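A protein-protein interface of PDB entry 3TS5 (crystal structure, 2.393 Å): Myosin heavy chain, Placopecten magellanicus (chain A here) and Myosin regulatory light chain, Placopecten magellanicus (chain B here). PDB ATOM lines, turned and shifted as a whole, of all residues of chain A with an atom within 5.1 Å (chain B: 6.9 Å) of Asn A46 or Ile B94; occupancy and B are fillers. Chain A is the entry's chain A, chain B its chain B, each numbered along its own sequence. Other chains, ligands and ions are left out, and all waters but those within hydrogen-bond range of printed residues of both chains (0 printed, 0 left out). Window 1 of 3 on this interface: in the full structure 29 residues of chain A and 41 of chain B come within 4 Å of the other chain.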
ATOM      1  N   SER A  41      10.340  27.954 -22.045  1.00  0.00           N
ATOM      2  CA  SER A  41      11.425  27.353 -22.788  1.00  0.00           C
ATOM      3  C   SER A  41      11.252  25.840 -22.875  1.00  0.00           C
ATOM      4  O   SER A  41      11.396  25.252 -23.960  1.00  0.00           O
ATOM      5  CB  SER A  41      12.760  27.688 -22.145  1.00  0.00           C
ATOM      6  OG  SER A  41      12.980  29.066 -22.247  1.00  0.00           O
ATOM      7  N   VAL A  42      10.951  25.223 -21.738  1.00  0.00           N
ATOM      8  CA  VAL A  42      10.660  23.789 -21.704  1.00  0.00           C
ATOM      9  C   VAL A  42       9.543  23.428 -22.679  1.00  0.00           C
ATOM     10  O   VAL A  42       9.661  22.489 -23.467  1.00  0.00           O
ATOM     11  CB  VAL A  42      10.238  23.343 -20.316  1.00  0.00           C
ATOM     12  CG1 VAL A  42       9.687  21.907 -20.356  1.00  0.00           C
ATOM     13  CG2 VAL A  42      11.403  23.480 -19.338  1.00  0.00           C
ATOM     14  N   ILE A  43       8.467  24.199 -22.627  1.00  0.00           N
ATOM     15  CA  ILE A  43       7.312  23.963 -23.478  1.00  0.00           C
ATOM     16  C   ILE A  43       7.611  24.096 -24.982  1.00  0.00           C
ATOM     17  O   ILE A  43       7.316  23.195 -25.749  1.00  0.00           O
ATOM     18  CB  ILE A  43       6.146  24.878 -23.056  1.00  0.00           C
ATOM     19  CG1 ILE A  43       5.639  24.474 -21.664  1.00  0.00           C
ATOM     20  CG2 ILE A  43       5.015  24.854 -24.093  1.00  0.00           C
ATOM     21  CD1 ILE A  43       4.669  25.501 -21.053  1.00  0.00           C
ATOM     22  N   GLN A  44       8.204  25.209 -25.392  1.00  0.00           N
ATOM     23  CA  GLN A  44       8.486  25.446 -26.807  1.00  0.00           C
ATOM     24  C   GLN A  44       9.453  24.405 -27.362  1.00  0.00           C
ATOM     25  O   GLN A  44       9.270  23.886 -28.477  1.00  0.00           O
ATOM     26  CB  GLN A  44       9.022  26.880 -27.030  1.00  0.00           C
ATOM     27  CG  GLN A  44       7.989  27.961 -26.666  1.00  0.00           C
ATOM     28  CD  GLN A  44       8.508  29.407 -26.742  1.00  0.00           C
ATOM     29  OE1 GLN A  44       9.616  29.729 -26.298  1.00  0.00           O
ATOM     30  NE2 GLN A  44       7.692  30.280 -27.317  1.00  0.00           N
ATOM     31  N   ARG A  45      10.473  24.109 -26.563  1.00  0.00           N
ATOM     32  CA  ARG A  45      11.534  23.185 -26.935  1.00  0.00           C
ATOM     33  C   ARG A  45      11.012  21.755 -27.108  1.00  0.00           C
ATOM     34  O   ARG A  45      11.295  21.089 -28.111  1.00  0.00           O
ATOM     35  CB  ARG A  45      12.596  23.204 -25.848  1.00  0.00           C
ATOM     36  CG  ARG A  45      13.652  22.135 -25.966  1.00  0.00           C
ATOM     37  CD  ARG A  45      14.775  22.407 -24.980  1.00  0.00           C
ATOM     38  NE  ARG A  45      14.455  22.011 -23.606  1.00  0.00           N
ATOM     39  CZ  ARG A  45      14.647  22.785 -22.541  1.00  0.00           C
ATOM     40  NH1 ARG A  45      15.119  24.024 -22.690  1.00  0.00           N
ATOM     41  NH2 ARG A  45      14.355  22.331 -21.327  1.00  0.00           N
ATOM     42  N   ASN A  46      10.233  21.299 -26.131  1.00  0.00           N
ATOM     43  CA  ASN A  46       9.609  19.989 -26.218  1.00  0.00           C
ATOM     44  C   ASN A  46       8.535  19.883 -27.294  1.00  0.00           C
ATOM     45  O   ASN A  46       8.385  18.835 -27.917  1.00  0.00           O
ATOM     46  CB  ASN A  46       9.079  19.537 -24.860  1.00  0.00           C
ATOM     47  CG  ASN A  46      10.189  19.066 -23.945  1.00  0.00           C
ATOM     48  OD1 ASN A  46      10.575  17.896 -23.970  1.00  0.00           O
ATOM     49  ND2 ASN A  46      10.724  19.983 -23.142  1.00  0.00           N
ATOM     50  N   ILE A  47       7.777  20.948 -27.530  1.00  0.00           N
ATOM     51  CA  ILE A  47       6.800  20.847 -28.594  1.00  0.00           C
ATOM     52  C   ILE A  47       7.556  20.748 -29.916  1.00  0.00           C
ATOM     53  O   ILE A  47       7.180  19.948 -30.792  1.00  0.00           O
ATOM     54  CB  ILE A  47       5.795  22.002 -28.625  1.00  0.00           C
ATOM     55  CG1 ILE A  47       4.854  21.934 -27.415  1.00  0.00           C
ATOM     56  CG2 ILE A  47       4.981  21.959 -29.925  1.00  0.00           C
ATOM     57  CD1 ILE A  47       4.002  23.194 -27.248  1.00  0.00           C
ATOM     58  N   ARG A  48       8.629  21.535 -30.041  1.00  0.00           N
ATOM     59  CA  ARG A  48       9.427  21.499 -31.262  1.00  0.00           C
ATOM     60  C   ARG A  48      10.085  20.127 -31.497  1.00  0.00           C
ATOM     61  O   ARG A  48      10.088  19.606 -32.631  1.00  0.00           O
ATOM     62  CB  ARG A  48      10.458  22.635 -31.310  1.00  0.00           C
ATOM     63  CG  ARG A  48       9.888  23.947 -31.854  1.00  0.00           C
ATOM     64  CD  ARG A  48      10.828  25.130 -31.625  1.00  0.00           C
ATOM     65  NE  ARG A  48      10.346  26.306 -32.350  1.00  0.00           N
ATOM     66  CZ  ARG A  48      10.313  27.556 -31.874  1.00  0.00           C
ATOM     67  NH1 ARG A  48      10.748  27.836 -30.627  1.00  0.00           N
ATOM     68  NH2 ARG A  48       9.833  28.533 -32.656  1.00  0.00           N
ATOM     69  N   LYS A  49      10.633  19.537 -30.434  1.00  0.00           N
ATOM     70  CA  LYS A  49      11.196  18.189 -30.537  1.00  0.00           C
ATOM     71  C   LYS A  49      10.125  17.202 -31.009  1.00  0.00           C
ATOM     72  O   LYS A  49      10.375  16.364 -31.887  1.00  0.00           O
ATOM     73  CB  LYS A  49      11.793  17.739 -29.203  1.00  0.00           C
ATOM     74  CG  LYS A  49      13.061  18.487 -28.811  1.00  0.00           C
ATOM     75  CD  LYS A  49      14.115  18.369 -29.894  1.00  0.00           C
ATOM     76  CE  LYS A  49      15.469  18.851 -29.401  1.00  0.00           C
ATOM     77  NZ  LYS A  49      16.510  18.720 -30.467  1.00  0.00           N
ATOM     78  N   TRP A  50       8.925  17.319 -30.439  1.00  0.00           N
ATOM     79  CA  TRP A  50       7.832  16.421 -30.794  1.00  0.00           C
ATOM     80  C   TRP A  50       7.481  16.484 -32.292  1.00  0.00           C
ATOM     81  O   TRP A  50       7.364  15.447 -32.944  1.00  0.00           O
ATOM     82  CB  TRP A  50       6.619  16.711 -29.921  1.00  0.00           C
ATOM     83  CG  TRP A  50       5.365  16.052 -30.368  1.00  0.00           C
ATOM     84  CD1 TRP A  50       5.066  14.715 -30.312  1.00  0.00           C
ATOM     85  CD2 TRP A  50       4.210  16.698 -30.905  1.00  0.00           C
ATOM     86  NE1 TRP A  50       3.801  14.492 -30.797  1.00  0.00           N
ATOM     87  CE2 TRP A  50       3.250  15.690 -31.167  1.00  0.00           C
ATOM     88  CE3 TRP A  50       3.889  18.034 -31.196  1.00  0.00           C
ATOM     89  CZ2 TRP A  50       1.989  15.975 -31.704  1.00  0.00           C
ATOM     90  CZ3 TRP A  50       2.635  18.315 -31.742  1.00  0.00           C
ATOM     91  CH2 TRP A  50       1.701  17.287 -31.984  1.00  0.00           C
ATOM     92  N   ARG B  16      24.231  19.286 -22.527  1.00  0.00           N
ATOM     93  CA  ARG B  16      23.632  17.974 -22.313  1.00  0.00           C
ATOM     94  C   ARG B  16      24.561  16.808 -22.634  1.00  0.00           C
ATOM     95  O   ARG B  16      25.770  16.990 -22.762  1.00  0.00           O
ATOM     96  CB  ARG B  16      22.196  17.948 -22.843  1.00  0.00           C
ATOM     97  CG  ARG B  16      21.132  18.073 -21.764  1.00  0.00           C
ATOM     98  CD  ARG B  16      19.744  18.229 -22.368  1.00  0.00           C
ATOM     99  NE  ARG B  16      19.014  19.350 -21.782  1.00  0.00           N
ATOM    100  CZ  ARG B  16      17.765  19.278 -21.331  1.00  0.00           C
ATOM    101  NH1 ARG B  16      17.099  18.135 -21.396  1.00  0.00           N
ATOM    102  NH2 ARG B  16      17.182  20.350 -20.816  1.00  0.00           N
ATOM    103  N   GLY B  87      17.204  17.859 -25.990  1.00  0.00           N
ATOM    104  CA  GLY B  87      16.635  18.771 -25.004  1.00  0.00           C
ATOM    105  C   GLY B  87      15.205  18.435 -24.610  1.00  0.00           C
ATOM    106  O   GLY B  87      14.407  19.335 -24.340  1.00  0.00           O
ATOM    107  N   THR B  88      14.868  17.146 -24.589  1.00  0.00           N
ATOM    108  CA  THR B  88      13.526  16.717 -24.202  1.00  0.00           C
ATOM    109  C   THR B  88      13.472  16.492 -22.713  1.00  0.00           C
ATOM    110  O   THR B  88      14.490  16.210 -22.083  1.00  0.00           O
ATOM    111  CB  THR B  88      13.080  15.439 -24.936  1.00  0.00           C
ATOM    112  OG1 THR B  88      13.839  14.313 -24.474  1.00  0.00           O
ATOM    113  CG2 THR B  88      13.280  15.607 -26.440  1.00  0.00           C
ATOM    114  N   ASP B  89      12.290  16.635 -22.137  1.00  0.00           N
ATOM    115  CA  ASP B  89      12.177  16.593 -20.689  1.00  0.00           C
ATOM    116  C   ASP B  89      11.105  15.601 -20.337  1.00  0.00           C
ATOM    117  O   ASP B  89      10.316  15.211 -21.199  1.00  0.00           O
ATOM    118  CB  ASP B  89      11.859  17.989 -20.137  1.00  0.00           C
ATOM    119  CG  ASP B  89      12.970  19.003 -20.430  1.00  0.00           C
ATOM    120  OD1 ASP B  89      13.977  18.993 -19.687  1.00  0.00           O
ATOM    121  OD2 ASP B  89      12.851  19.806 -21.402  1.00  0.00           O
ATOM    122  N   SER B  90      11.068  15.175 -19.080  1.00  0.00           N
ATOM    123  CA  SER B  90      10.047  14.210 -18.665  1.00  0.00           C
ATOM    124  C   SER B  90       8.641  14.803 -18.751  1.00  0.00           C
ATOM    125  O   SER B  90       8.448  16.036 -18.718  1.00  0.00           O
ATOM    126  CB  SER B  90      10.310  13.691 -17.242  1.00  0.00           C
ATOM    127  OG  SER B  90      10.114  14.716 -16.284  1.00  0.00           O
ATOM    128  N   GLU B  91       7.669  13.904 -18.873  1.00  0.00           N
ATOM    129  CA  GLU B  91       6.259  14.251 -18.773  1.00  0.00           C
ATOM    130  C   GLU B  91       6.050  15.174 -17.567  1.00  0.00           C
ATOM    131  O   GLU B  91       5.371  16.203 -17.665  1.00  0.00           O
ATOM    132  CB  GLU B  91       5.444  12.964 -18.628  1.00  0.00           C
ATOM    133  CG  GLU B  91       3.920  13.120 -18.692  1.00  0.00           C
ATOM    134  CD  GLU B  91       3.291  12.184 -19.729  1.00  0.00           C
ATOM    135  OE1 GLU B  91       3.913  12.008 -20.804  1.00  0.00           O
ATOM    136  OE2 GLU B  91       2.191  11.624 -19.474  1.00  0.00           O
ATOM    137  N   GLU B  92       6.663  14.813 -16.439  1.00  0.00           N
ATOM    138  CA  GLU B  92       6.525  15.578 -15.210  1.00  0.00           C
ATOM    139  C   GLU B  92       7.019  17.012 -15.369  1.00  0.00           C
ATOM    140  O   GLU B  92       6.313  17.973 -15.049  1.00  0.00           O
ATOM    141  CB  GLU B  92       7.318  14.889 -14.102  1.00  0.00           C
ATOM    142  CG  GLU B  92       6.866  15.234 -12.699  1.00  0.00           C
ATOM    143  CD  GLU B  92       7.547  14.367 -11.646  1.00  0.00           C
ATOM    144  OE1 GLU B  92       8.801  14.428 -11.541  1.00  0.00           O
ATOM    145  OE2 GLU B  92       6.828  13.619 -10.940  1.00  0.00           O
ATOM    146  N   THR B  93       8.251  17.150 -15.846  1.00  0.00           N
ATOM    147  CA  THR B  93       8.853  18.458 -16.025  1.00  0.00           C
ATOM    148  C   THR B  93       7.981  19.344 -16.916  1.00  0.00           C
ATOM    149  O   THR B  93       7.760  20.518 -16.604  1.00  0.00           O
ATOM    150  CB  THR B  93      10.267  18.334 -16.616  1.00  0.00           C
ATOM    151  OG1 THR B  93      11.031  17.450 -15.793  1.00  0.00           O
ATOM    152  CG2 THR B  93      10.976  19.703 -16.695  1.00  0.00           C
ATOM    153  N   ILE B  94       7.457  18.776 -17.998  1.00  0.00           N
ATOM    154  CA  ILE B  94       6.663  19.563 -18.918  1.00  0.00           C
ATOM    155  C   ILE B  94       5.318  19.975 -18.309  1.00  0.00           C
ATOM    156  O   ILE B  94       4.898  21.118 -18.463  1.00  0.00           O
ATOM    157  CB  ILE B  94       6.474  18.877 -20.281  1.00  0.00           C
ATOM    158  CG1 ILE B  94       7.836  18.501 -20.884  1.00  0.00           C
ATOM    159  CG2 ILE B  94       5.733  19.804 -21.206  1.00  0.00           C
ATOM    160  CD1 ILE B  94       7.756  17.578 -22.123  1.00  0.00           C
ATOM    161  N   ARG B  95       4.651  19.046 -17.629  1.00  0.00           N
ATOM    162  CA  ARG B  95       3.461  19.380 -16.846  1.00  0.00           C
ATOM    163  C   ARG B  95       3.709  20.519 -15.846  1.00  0.00           C
ATOM    164  O   ARG B  95       2.881  21.412 -15.695  1.00  0.00           O
ATOM    165  CB  ARG B  95       2.922  18.154 -16.106  1.00  0.00           C
ATOM    166  CG  ARG B  95       1.869  17.376 -16.879  1.00  0.00           C
ATOM    167  CD  ARG B  95       1.247  16.273 -16.031  1.00  0.00           C
ATOM    168  NE  ARG B  95       1.978  15.026 -16.205  1.00  0.00           N
ATOM    169  CZ  ARG B  95       2.766  14.484 -15.285  1.00  0.00           C
ATOM    170  NH1 ARG B  95       2.907  15.069 -14.097  1.00  0.00           N
ATOM    171  NH2 ARG B  95       3.399  13.350 -15.555  1.00  0.00           N
ATOM    172  N   ASN B  96       4.845  20.502 -15.166  1.00  0.00           N
ATOM    173  CA  ASN B  96       5.127  21.575 -14.223  1.00  0.00           C
ATOM    174  C   ASN B  96       5.449  22.897 -14.913  1.00  0.00           C
ATOM    175  O   ASN B  96       5.168  23.985 -14.369  1.00  0.00           O
ATOM    176  CB  ASN B  96       6.206  21.159 -13.214  1.00  0.00           C
ATOM    177  CG  ASN B  96       5.805  19.894 -12.443  1.00  0.00           C
ATOM    178  OD1 ASN B  96       4.611  19.653 -12.207  1.00  0.00           O
ATOM    179  ND2 ASN B  96       6.793  19.075 -12.074  1.00  0.00           N
ATOM    180  N   ALA B  97       6.017  22.795 -16.114  1.00  0.00           N
ATOM    181  CA  ALA B  97       6.275  23.954 -16.963  1.00  0.00           C
ATOM    182  C   ALA B  97       4.953  24.644 -17.260  1.00  0.00           C
ATOM    183  O   ALA B  97       4.813  25.857 -17.081  1.00  0.00           O
ATOM    184  CB  ALA B  97       6.975  23.522 -18.281  1.00  0.00           C
ATOM    185  N   PHE B  98       3.983  23.862 -17.725  1.00  0.00           N
ATOM    186  CA  PHE B  98       2.635  24.365 -17.934  1.00  0.00           C
ATOM    187  C   PHE B  98       2.000  24.885 -16.624  1.00  0.00           C
ATOM    188  O   PHE B  98       1.299  25.910 -16.616  1.00  0.00           O
ATOM    189  CB  PHE B  98       1.747  23.287 -18.551  1.00  0.00           C
ATOM    190  CG  PHE B  98       1.906  23.135 -20.038  1.00  0.00           C
ATOM    191  CD1 PHE B  98       1.452  24.117 -20.907  1.00  0.00           C
ATOM    192  CD2 PHE B  98       2.468  21.977 -20.581  1.00  0.00           C
ATOM    193  CE1 PHE B  98       1.564  23.959 -22.296  1.00  0.00           C
ATOM    194  CE2 PHE B  98       2.596  21.811 -21.971  1.00  0.00           C
ATOM    195  CZ  PHE B  98       2.140  22.794 -22.828  1.00  0.00           C
ATOM    196  N   GLY B  99       2.248  24.170 -15.530  1.00  0.00           N
ATOM    197  CA  GLY B  99       1.666  24.494 -14.236  1.00  0.00           C
ATOM    198  C   GLY B  99       2.064  25.886 -13.766  1.00  0.00           C
ATOM    199  O   GLY B  99       1.370  26.516 -12.982  1.00  0.00           O
ATOM    200  N   PHE B 125       6.861  30.974 -31.859  1.00  0.00           N
ATOM    201  CA  PHE B 125       6.489  29.961 -32.844  1.00  0.00           C
ATOM    202  C   PHE B 125       6.078  30.674 -34.112  1.00  0.00           C
ATOM    203  O   PHE B 125       5.353  31.674 -34.045  1.00  0.00           O
ATOM    204  CB  PHE B 125       5.299  29.119 -32.369  1.00  0.00           C
ATOM    205  CG  PHE B 125       5.682  27.900 -31.602  1.00  0.00           C
ATOM    206  CD1 PHE B 125       6.885  27.838 -30.927  1.00  0.00           C
ATOM    207  CD2 PHE B 125       4.827  26.806 -31.553  1.00  0.00           C
ATOM    208  CE1 PHE B 125       7.234  26.705 -30.202  1.00  0.00           C
ATOM    209  CE2 PHE B 125       5.164  25.674 -30.840  1.00  0.00           C
ATOM    210  CZ  PHE B 125       6.372  25.622 -30.160  1.00  0.00           C
ATOM    211  N   TYR B 146      -3.467  20.771 -20.945  1.00  0.00           N
ATOM    212  CA  TYR B 146      -2.037  20.549 -21.090  1.00  0.00           C
ATOM    213  C   TYR B 146      -1.547  19.206 -20.562  1.00  0.00           C
ATOM    214  O   TYR B 146      -0.568  18.653 -21.075  1.00  0.00           O
ATOM    215  CB  TYR B 146      -1.223  21.711 -20.512  1.00  0.00           C
ATOM    216  CG  TYR B 146      -1.317  21.952 -19.016  1.00  0.00           C
ATOM    217  CD1 TYR B 146      -0.653  21.125 -18.113  1.00  0.00           C
ATOM    218  CD2 TYR B 146      -2.008  23.053 -18.511  1.00  0.00           C
ATOM    219  CE1 TYR B 146      -0.706  21.362 -16.740  1.00  0.00           C
ATOM    220  CE2 TYR B 146      -2.066  23.312 -17.139  1.00  0.00           C
ATOM    221  CZ  TYR B 146      -1.409  22.459 -16.259  1.00  0.00           C
ATOM    222  OH  TYR B 146      -1.451  22.690 -14.904  1.00  0.00           O
ATOM    223  N   PHE B 149      -2.308  17.134 -23.333  1.00  0.00           N
ATOM    224  CA  PHE B 149      -1.372  17.527 -24.380  1.00  0.00           C
ATOM    225  C   PHE B 149       0.025  16.933 -24.147  1.00  0.00           C
ATOM    226  O   PHE B 149       0.688  16.514 -25.089  1.00  0.00           O
ATOM    227  CB  PHE B 149      -1.314  19.058 -24.499  1.00  0.00           C
ATOM    228  CG  PHE B 149      -0.356  19.548 -25.541  1.00  0.00           C
ATOM    229  CD1 PHE B 149      -0.721  19.573 -26.875  1.00  0.00           C
ATOM    230  CD2 PHE B 149       0.917  19.978 -25.180  1.00  0.00           C
ATOM    231  CE1 PHE B 149       0.156  20.026 -27.840  1.00  0.00           C
ATOM    232  CE2 PHE B 149       1.795  20.431 -26.127  1.00  0.00           C
ATOM    233  CZ  PHE B 149       1.419  20.456 -27.464  1.00  0.00           C
ATOM    234  N   VAL B 150       0.457  16.888 -22.891  1.00  0.00           N
ATOM    235  CA  VAL B 150       1.766  16.363 -22.548  1.00  0.00           C
ATOM    236  C   VAL B 150       1.831  14.852 -22.767  1.00  0.00           C
ATOM    237  O   VAL B 150       2.840  14.334 -23.231  1.00  0.00           O
ATOM    238  CB  VAL B 150       2.182  16.723 -21.111  1.00  0.00           C
ATOM    239  CG1 VAL B 150       3.413  15.923 -20.710  1.00  0.00           C
ATOM    240  CG2 VAL B 150       2.479  18.224 -20.993  1.00  0.00           C
ATOM    241  N   ILE B 153       2.272  14.363 -26.628  1.00  0.00           N
ATOM    242  CA  ILE B 153       3.558  14.614 -27.261  1.00  0.00           C
ATOM    243  C   ILE B 153       4.642  13.639 -26.812  1.00  0.00           C
ATOM    244  O   ILE B 153       5.714  13.578 -27.423  1.00  0.00           O
ATOM    245  CB  ILE B 153       4.034  16.062 -27.105  1.00  0.00           C
ATOM    246  CG1 ILE B 153       4.362  16.387 -25.649  1.00  0.00           C
ATOM    247  CG2 ILE B 153       3.005  17.021 -27.692  1.00  0.00           C
ATOM    248  CD1 ILE B 153       4.820  17.837 -25.433  1.00  0.00           C
ATOM    249  N   LYS B 154       4.361  12.872 -25.761  1.00  0.00           N
ATOM    250  CA  LYS B 154       5.298  11.851 -25.321  1.00  0.00           C
ATOM    251  C   LYS B 154       4.962  10.487 -25.900  1.00  0.00           C
ATOM    252  O   LYS B 154       5.823   9.621 -25.968  1.00  0.00           O
ATOM    253  CB  LYS B 154       5.335  11.763 -23.795  1.00  0.00           C
ATOM    254  CG  LYS B 154       5.833  13.024 -23.104  1.00  0.00           C
ATOM    255  CD  LYS B 154       7.216  13.416 -23.596  1.00  0.00           C
ATOM    256  CE  LYS B 154       8.264  13.116 -22.529  1.00  0.00           C
ATOM    257  NZ  LYS B 154       9.645  13.405 -23.009  1.00  0.00           N
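NH2 of Arg B16 lies within salt-bridge range of OD1 of Asp B89.
O of Asp B89 lies within hydrogen-bond range of NZ of Lys B154, at 2.6 Å.
The backbone carbonyl oxygen (O) of Val A42 sits at hydrogen-bond distance from the side-chain amide nitrogen (ND2) of Asn A46.
The backbone carbonyl oxygen (O) of Thr B88 is in hydrogen-bond range of the guanidinium group (NH1) of Arg B16 (3.3 Å).
The guanidinium group of Arg B16 lies close to the guanidinium group of Arg A45, at 3.5 Å.
NE of Arg A45 lies within hydrogen-bond range of O of Gly B87, at 2.8 Å.
The guanidinium group (NH2) of Arg A45 lies within salt-bridge range of the side-chain carboxylate (OD2) of Asp B89 (2.9 Å).
The side-chain amide nitrogen (ND2) of Asn A46 sits at hydrogen-bond distance from the side-chain carboxylate (OD2) of Asp B89 (2.8 Å).
Printed residues of chain B within 4 Å of Val A42: Asp B89, Ile B94 and Ala B97.
Asn A46 touches four residues of chain B.
Of the printed residues of chain B, Arg A48 touches Phe B125 (3.5 Å).
Of chain A, only Val A42 and Asn A46 come within 4 Å of Ile B94.
Printed residues of chain A within 4 Å of Ala B97: Val A42 and Ile A43.
Printed residues of chain A within 4 Å of Phe B125: Gln A44 (3.6 Å), Ile A47 (3.8 Å) and Arg A48 (3.5 Å).
Hydrophobic or aromatic side chains of chain B that line the printed part of chain A: Ile B94, Ala B97, Phe B98, Phe B125, Phe B149 and Ile B153.
Printed residues of chain A that touch a printed residue of chain B: Val A42, Ile A43, Gln A44, Arg A45, Asn A46, Ile A47, Arg A48, Lys A49 and Trp A50.
Hydrophobic or aromatic side chains of chain A that line the printed part of chain B: Val A42, Ile A43, Ile A47 and Trp A50.
Among the printed residues, Asp or Glu carboxylates within 4 Å of a Lys or Arg side-chain nitrogen of the other chain: Arg A45 with Asp B89.
CG1 of Ile B94 touches CG1 of Val A42, 3.9 Å away.
Ala B97 touches Val A42 (CB to CG1, 3.8 Å).
Ala B97 touches Ile A43.
Ile A43 touches Phe B98 (CD1 to CD1, 3.5 Å).
Gln A44 touches Phe B125.
ND2 of Asn A46 touches O of Gly B87, at 3.9 Å.
CD1 of Ile B94 touches CG of Asn A46, 3.4 Å away.
Ile A47 touches Phe B125.
Lys A49 touches Gly B87.
Lys A49 touches Thr B88 (CG to CG2, 3.7 Å).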
